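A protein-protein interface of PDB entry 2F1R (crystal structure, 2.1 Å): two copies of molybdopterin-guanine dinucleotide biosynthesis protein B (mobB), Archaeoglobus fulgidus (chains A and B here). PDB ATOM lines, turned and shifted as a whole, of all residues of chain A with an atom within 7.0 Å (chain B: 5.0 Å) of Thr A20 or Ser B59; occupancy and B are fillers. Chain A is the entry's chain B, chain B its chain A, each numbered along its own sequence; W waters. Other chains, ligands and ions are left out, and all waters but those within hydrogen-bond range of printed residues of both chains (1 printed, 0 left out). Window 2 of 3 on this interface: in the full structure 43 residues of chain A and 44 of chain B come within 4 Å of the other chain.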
ATOM      1  N   LYS A  15       1.813 -19.996 -16.829  1.00  0.00           N
ATOM      2  CA  LYS A  15       2.012 -19.423 -15.504  1.00  0.00           C
ATOM      3  C   LYS A  15       1.635 -20.407 -14.413  1.00  0.00           C
ATOM      4  O   LYS A  15       2.427 -20.616 -13.505  1.00  0.00           O
ATOM      5  CB  LYS A  15       1.183 -18.135 -15.315  1.00  0.00           C
ATOM      6  CG  LYS A  15       1.322 -17.069 -16.380  1.00  0.00           C
ATOM      7  CD  LYS A  15       0.438 -15.899 -16.017  1.00  0.00           C
ATOM      8  CE  LYS A  15      -0.971 -16.024 -16.609  1.00  0.00           C
ATOM      9  NZ  LYS A  15      -1.843 -14.930 -16.062  1.00  0.00           N
ATOM     10  N   THR A  16       0.427 -20.993 -14.523  1.00  0.00           N
ATOM     11  CA  THR A  16      -0.072 -21.997 -13.552  1.00  0.00           C
ATOM     12  C   THR A  16       0.811 -23.226 -13.421  1.00  0.00           C
ATOM     13  O   THR A  16       1.175 -23.635 -12.311  1.00  0.00           O
ATOM     14  CB  THR A  16      -1.536 -22.475 -13.882  1.00  0.00           C
ATOM     15  OG1 THR A  16      -2.392 -21.343 -13.956  1.00  0.00           O
ATOM     16  CG2 THR A  16      -2.076 -23.458 -12.801  1.00  0.00           C
ATOM     17  N   THR A  17       1.131 -23.850 -14.550  1.00  0.00           N
ATOM     18  CA  THR A  17       2.059 -24.994 -14.522  1.00  0.00           C
ATOM     19  C   THR A  17       3.373 -24.630 -13.809  1.00  0.00           C
ATOM     20  O   THR A  17       3.895 -25.403 -13.017  1.00  0.00           O
ATOM     21  CB  THR A  17       2.298 -25.480 -15.954  1.00  0.00           C
ATOM     22  OG1 THR A  17       1.011 -25.755 -16.521  1.00  0.00           O
ATOM     23  CG2 THR A  17       3.147 -26.735 -16.004  1.00  0.00           C
ATOM     24  N   LEU A  18       3.909 -23.438 -14.066  1.00  0.00           N
ATOM     25  CA  LEU A  18       5.197 -23.082 -13.460  1.00  0.00           C
ATOM     26  C   LEU A  18       5.026 -23.002 -11.936  1.00  0.00           C
ATOM     27  O   LEU A  18       5.764 -23.643 -11.179  1.00  0.00           O
ATOM     28  CB  LEU A  18       5.754 -21.753 -14.007  1.00  0.00           C
ATOM     29  CG  LEU A  18       7.108 -21.315 -13.403  1.00  0.00           C
ATOM     30  CD1 LEU A  18       8.164 -22.373 -13.566  1.00  0.00           C
ATOM     31  CD2 LEU A  18       7.613 -19.947 -13.874  1.00  0.00           C
ATOM     32  N   ILE A  19       4.034 -22.238 -11.508  1.00  0.00           N
ATOM     33  CA  ILE A  19       3.753 -22.101 -10.076  1.00  0.00           C
ATOM     34  C   ILE A  19       3.562 -23.461  -9.388  1.00  0.00           C
ATOM     35  O   ILE A  19       4.227 -23.759  -8.376  1.00  0.00           O
ATOM     36  CB  ILE A  19       2.575 -21.131  -9.837  1.00  0.00           C
ATOM     37  CG1 ILE A  19       2.949 -19.720 -10.369  1.00  0.00           C
ATOM     38  CG2 ILE A  19       2.198 -21.154  -8.340  1.00  0.00           C
ATOM     39  CD1 ILE A  19       1.788 -18.748 -10.527  1.00  0.00           C
ATOM     40  N   THR A  20       2.721 -24.312  -9.989  1.00  0.00           N
ATOM     41  CA  THR A  20       2.355 -25.567  -9.340  1.00  0.00           C
ATOM     42  C   THR A  20       3.553 -26.492  -9.365  1.00  0.00           C
ATOM     43  O   THR A  20       3.823 -27.201  -8.365  1.00  0.00           O
ATOM     44  CB  THR A  20       1.083 -26.241  -9.951  1.00  0.00           C
ATOM     45  OG1 THR A  20       1.230 -26.365 -11.369  1.00  0.00           O
ATOM     46  CG2 THR A  20      -0.165 -25.371  -9.653  1.00  0.00           C
ATOM     47  N   ARG A  21       4.331 -26.440 -10.455  1.00  0.00           N
ATOM     48  CA  ARG A  21       5.500 -27.333 -10.497  1.00  0.00           C
ATOM     49  C   ARG A  21       6.612 -26.874  -9.594  1.00  0.00           C
ATOM     50  O   ARG A  21       7.272 -27.698  -9.018  1.00  0.00           O
ATOM     51  CB  ARG A  21       5.948 -27.707 -11.939  1.00  0.00           C
ATOM     52  CG  ARG A  21       4.842 -28.492 -12.739  1.00  0.00           C
ATOM     53  CD  ARG A  21       5.371 -29.005 -14.096  1.00  0.00           C
ATOM     54  NE  ARG A  21       6.321 -30.071 -13.787  1.00  0.00           N
ATOM     55  CZ  ARG A  21       7.562 -30.152 -14.245  1.00  0.00           C
ATOM     56  NH1 ARG A  21       8.017 -29.291 -15.157  1.00  0.00           N
ATOM     57  NH2 ARG A  21       8.315 -31.136 -13.803  1.00  0.00           N
ATOM     58  N   MET A  22       6.813 -25.553  -9.437  1.00  0.00           N
ATOM     59  CA  MET A  22       7.820 -25.023  -8.464  1.00  0.00           C
ATOM     60  C   MET A  22       7.418 -25.246  -6.989  1.00  0.00           C
ATOM     61  O   MET A  22       8.289 -25.305  -6.112  1.00  0.00           O
ATOM     62  CB  MET A  22       7.997 -23.504  -8.646  1.00  0.00           C
ATOM     63  CG  MET A  22       8.799 -23.031  -9.907  1.00  0.00           C
ATOM     64  SD  MET A  22       9.128 -21.241  -9.742  1.00  0.00           S
ATOM     65  CE  MET A  22       7.485 -20.551  -9.483  1.00  0.00           C
ATOM     66  N   MET A  23       6.105 -25.378  -6.717  1.00  0.00           N
ATOM     67  CA  MET A  23       5.586 -25.318  -5.350  1.00  0.00           C
ATOM     68  C   MET A  23       6.149 -26.336  -4.374  1.00  0.00           C
ATOM     69  O   MET A  23       6.539 -25.946  -3.267  1.00  0.00           O
ATOM     70  CB  MET A  23       4.055 -25.259  -5.301  1.00  0.00           C
ATOM     71  CG  MET A  23       3.465 -24.843  -3.887  1.00  0.00           C
ATOM     72  SD  MET A  23       3.902 -23.136  -3.463  1.00  0.00           S
ATOM     73  CE  MET A  23       3.408 -22.365  -4.988  1.00  0.00           C
ATOM     74  N   PRO A  24       6.230 -27.626  -4.774  1.00  0.00           N
ATOM     75  CA  PRO A  24       6.878 -28.654  -3.905  1.00  0.00           C
ATOM     76  C   PRO A  24       8.302 -28.300  -3.517  1.00  0.00           C
ATOM     77  O   PRO A  24       8.699 -28.506  -2.373  1.00  0.00           O
ATOM     78  CB  PRO A  24       6.904 -29.924  -4.775  1.00  0.00           C
ATOM     79  CG  PRO A  24       5.849 -29.703  -5.854  1.00  0.00           C
ATOM     80  CD  PRO A  24       5.672 -28.206  -6.019  1.00  0.00           C
ATOM     81  N   ILE A  25       9.082 -27.771  -4.453  1.00  0.00           N
ATOM     82  CA  ILE A  25      10.427 -27.320  -4.132  1.00  0.00           C
ATOM     83  C   ILE A  25      10.457 -26.141  -3.150  1.00  0.00           C
ATOM     84  O   ILE A  25      11.252 -26.137  -2.205  1.00  0.00           O
ATOM     85  CB  ILE A  25      11.240 -26.987  -5.451  1.00  0.00           C
ATOM     86  CG1 ILE A  25      11.377 -28.228  -6.354  1.00  0.00           C
ATOM     87  CG2 ILE A  25      12.633 -26.365  -5.139  1.00  0.00           C
ATOM     88  CD1 ILE A  25      11.170 -27.919  -7.808  1.00  0.00           C
ATOM     89  N   ARG A  27       8.210 -25.331  -0.936  1.00  0.00           N
ATOM     90  CA  ARG A  27       7.676 -25.789   0.359  1.00  0.00           C
ATOM     91  C   ARG A  27       8.639 -26.733   1.077  1.00  0.00           C
ATOM     92  O   ARG A  27       8.787 -26.666   2.280  1.00  0.00           O
ATOM     93  CB  ARG A  27       6.317 -26.464   0.179  1.00  0.00           C
ATOM     94  CG  ARG A  27       5.286 -25.606  -0.530  1.00  0.00           C
ATOM     95  CD  ARG A  27       4.089 -25.267   0.289  1.00  0.00           C
ATOM     96  NE  ARG A  27       4.451 -24.820   1.626  1.00  0.00           N
ATOM     97  CZ  ARG A  27       4.028 -25.400   2.751  1.00  0.00           C
ATOM     98  NH1 ARG A  27       3.187 -26.443   2.705  1.00  0.00           N
ATOM     99  NH2 ARG A  27       4.452 -24.935   3.925  1.00  0.00           N
ATOM    100  N   VAL A  35      -0.655 -17.775  -2.903  1.00  0.00           N
ATOM    101  CA  VAL A  35      -0.787 -17.273  -4.257  1.00  0.00           C
ATOM    102  C   VAL A  35      -2.057 -16.461  -4.363  1.00  0.00           C
ATOM    103  O   VAL A  35      -3.132 -16.952  -4.014  1.00  0.00           O
ATOM    104  CB  VAL A  35      -0.839 -18.423  -5.295  1.00  0.00           C
ATOM    105  CG1 VAL A  35      -1.179 -17.905  -6.700  1.00  0.00           C
ATOM    106  CG2 VAL A  35       0.504 -19.222  -5.314  1.00  0.00           C
ATOM    107  N   VAL A 149      12.203 -25.687 -13.818  1.00  0.00           N
ATOM    108  CA  VAL A 149      11.424 -25.379 -12.625  1.00  0.00           C
ATOM    109  C   VAL A 149      12.322 -25.299 -11.395  1.00  0.00           C
ATOM    110  O   VAL A 149      12.173 -24.451 -10.540  1.00  0.00           O
ATOM    111  CB  VAL A 149      10.304 -26.413 -12.400  1.00  0.00           C
ATOM    112  CG1 VAL A 149       9.958 -26.509 -10.922  1.00  0.00           C
ATOM    113  CG2 VAL A 149       9.077 -26.055 -13.222  1.00  0.00           C
ATOM    114  N   LYS B  55      -5.817 -26.399  -8.529  1.00  0.00           N
ATOM    115  CA  LYS B  55      -4.463 -26.918  -8.824  1.00  0.00           C
ATOM    116  C   LYS B  55      -3.367 -26.266  -7.988  1.00  0.00           C
ATOM    117  O   LYS B  55      -2.480 -26.949  -7.464  1.00  0.00           O
ATOM    118  CB  LYS B  55      -4.113 -26.681 -10.286  1.00  0.00           C
ATOM    119  CG  LYS B  55      -4.661 -27.693 -11.191  1.00  0.00           C
ATOM    120  CD  LYS B  55      -4.616 -27.204 -12.623  1.00  0.00           C
ATOM    121  CE  LYS B  55      -5.770 -27.800 -13.446  1.00  0.00           C
ATOM    122  NZ  LYS B  55      -5.455 -27.742 -14.895  1.00  0.00           N
ATOM    123  N   ILE B  56      -3.388 -24.941  -7.904  1.00  0.00           N
ATOM    124  CA  ILE B  56      -2.406 -24.227  -7.076  1.00  0.00           C
ATOM    125  C   ILE B  56      -2.573 -24.678  -5.599  1.00  0.00           C
ATOM    126  O   ILE B  56      -1.611 -25.053  -4.933  1.00  0.00           O
ATOM    127  CB  ILE B  56      -2.495 -22.672  -7.266  1.00  0.00           C
ATOM    128  CG1 ILE B  56      -1.991 -22.273  -8.661  1.00  0.00           C
ATOM    129  CG2 ILE B  56      -1.648 -21.968  -6.213  1.00  0.00           C
ATOM    130  CD1 ILE B  56      -2.707 -21.106  -9.311  1.00  0.00           C
ATOM    131  N   TYR B  57      -3.812 -24.662  -5.110  1.00  0.00           N
ATOM    132  CA  TYR B  57      -4.062 -25.131  -3.771  1.00  0.00           C
ATOM    133  C   TYR B  57      -3.461 -26.526  -3.507  1.00  0.00           C
ATOM    134  O   TYR B  57      -2.714 -26.708  -2.547  1.00  0.00           O
ATOM    135  CB  TYR B  57      -5.540 -25.132  -3.408  1.00  0.00           C
ATOM    136  CG  TYR B  57      -5.693 -25.484  -1.954  1.00  0.00           C
ATOM    137  CD1 TYR B  57      -5.606 -24.498  -0.987  1.00  0.00           C
ATOM    138  CD2 TYR B  57      -5.839 -26.804  -1.539  1.00  0.00           C
ATOM    139  CE1 TYR B  57      -5.733 -24.793   0.372  1.00  0.00           C
ATOM    140  CE2 TYR B  57      -5.951 -27.119  -0.189  1.00  0.00           C
ATOM    141  CZ  TYR B  57      -5.904 -26.093   0.760  1.00  0.00           C
ATOM    142  OH  TYR B  57      -6.020 -26.348   2.094  1.00  0.00           O
ATOM    143  N   ASN B  58      -3.758 -27.482  -4.393  1.00  0.00           N
ATOM    144  CA  ASN B  58      -3.226 -28.860  -4.288  1.00  0.00           C
ATOM    145  C   ASN B  58      -1.710 -28.986  -4.279  1.00  0.00           C
ATOM    146  O   ASN B  58      -1.146 -29.863  -3.628  1.00  0.00           O
ATOM    147  CB  ASN B  58      -3.784 -29.700  -5.432  1.00  0.00           C
ATOM    148  CG  ASN B  58      -5.131 -30.289  -5.106  1.00  0.00           C
ATOM    149  OD1 ASN B  58      -5.998 -29.615  -4.528  1.00  0.00           O
ATOM    150  ND2 ASN B  58      -5.328 -31.567  -5.466  1.00  0.00           N
ATOM    151  N   SER B  59      -1.052 -28.082  -5.002  1.00  0.00           N
ATOM    152  CA  SER B  59       0.393 -28.085  -5.123  1.00  0.00           C
ATOM    153  C   SER B  59       1.041 -27.628  -3.819  1.00  0.00           C
ATOM    154  O   SER B  59       2.246 -27.784  -3.608  1.00  0.00           O
ATOM    155  CB  SER B  59       0.807 -27.202  -6.315  1.00  0.00           C
ATOM    156  OG  SER B  59       0.670 -25.802  -6.010  1.00  0.00           O
ATOM    157  N   GLY B  60       0.249 -27.096  -2.905  1.00  0.00           N
ATOM    158  CA  GLY B  60       0.830 -26.737  -1.621  1.00  0.00           C
ATOM    159  C   GLY B  60       0.812 -25.267  -1.260  1.00  0.00           C
ATOM    160  O   GLY B  60       1.385 -24.887  -0.229  1.00  0.00           O
ATOM    161  N   ALA B  61       0.153 -24.439  -2.076  1.00  0.00           N
ATOM    162  CA  ALA B  61      -0.041 -23.004  -1.766  1.00  0.00           C
ATOM    163  C   ALA B  61      -1.420 -22.753  -1.174  1.00  0.00           C
ATOM    164  O   ALA B  61      -2.402 -23.383  -1.605  1.00  0.00           O
ATOM    165  CB  ALA B  61       0.155 -22.092  -3.022  1.00  0.00           C
HETATM  166  O   HOH W   1       1.955 -22.972   1.727  1.00  0.00           O
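Water W1 bridges the backbone carbonyl oxygen (O) of Gly B60 and the guanidinium group (NE) of Arg A27.
No position is printed for both chains.
Of the 9 pairs that touch across the chains among the printed residues, none has its exchanged pair printed and touching as well.
Of the 7 printed residues of chain B, 5 touch a printed residue of chain A.
Hydrophobic or aromatic side chains of chain B within 4 Å of the printed part of chain A: Ile B56 and Ala B61.
Hydrophobic or aromatic side chains of chain A that line the printed part of chain B: Met A23 and Val A35.
Among the printed residues, 9 pairs touch across the chains.
Among the printed residues, merely in contact across the chains: Thr A20 with Lys B55 (3.6 Å), Thr A20 with Ile B56 (3.6 Å), Thr A20 with Ser B59 (3.6 Å), Met A23 with Ser B59 (3.2 Å), Met A23 with Gly B60 (3.8 Å), Met A23 with Ala B61 (3.8 Å), Arg A27 with Gly B60 (2.8 Å), Val A35 with Ile B56 (3.6 Å) and Val A35 with Ala B61 (3.7 Å).
Thr A20 touches three residues of chain B.
Ser B59 touches just these residues of chain A: Thr A20 (3.6 Å) and Met A23 (3.2 Å).
Of the printed residues of chain A, Ala B61 touches Met A23 and Val A35.
Of the printed residues of chain A, Gly B60 touches Met A23 and Arg A27.
Printed residues of chain A within 4 Å of Lys B55: Thr A20.
Ile A19 touches none of the printed residues of chain B.
Asn B58 touches none of the printed residues of chain A.
The nearest printed residue of chain B that does not touch Thr A20 is Tyr B57 (5.9 Å).
The nearest residue of chain A that does not touch Ser B59 is Pro A24 (4.2 Å).
The nearest printed residue of chain A that does not touch Lys B55 is Thr A16 (4.5 Å).
OG1 of Thr A20 sits at hydrogen-bond distance from O of Thr A17 (3.3 Å).
The backbone carbonyl oxygen of Ile B56 is in hydrogen-bond range of the backbone NH of Ala B61 (3.4 Å).
OG1 of Thr A20 sits at hydrogen-bond distance from O of Thr A16 (2.9 Å).
OG of Ser B59 lies within hydrogen-bond range of O of Ile B56, 2.6 Å away.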
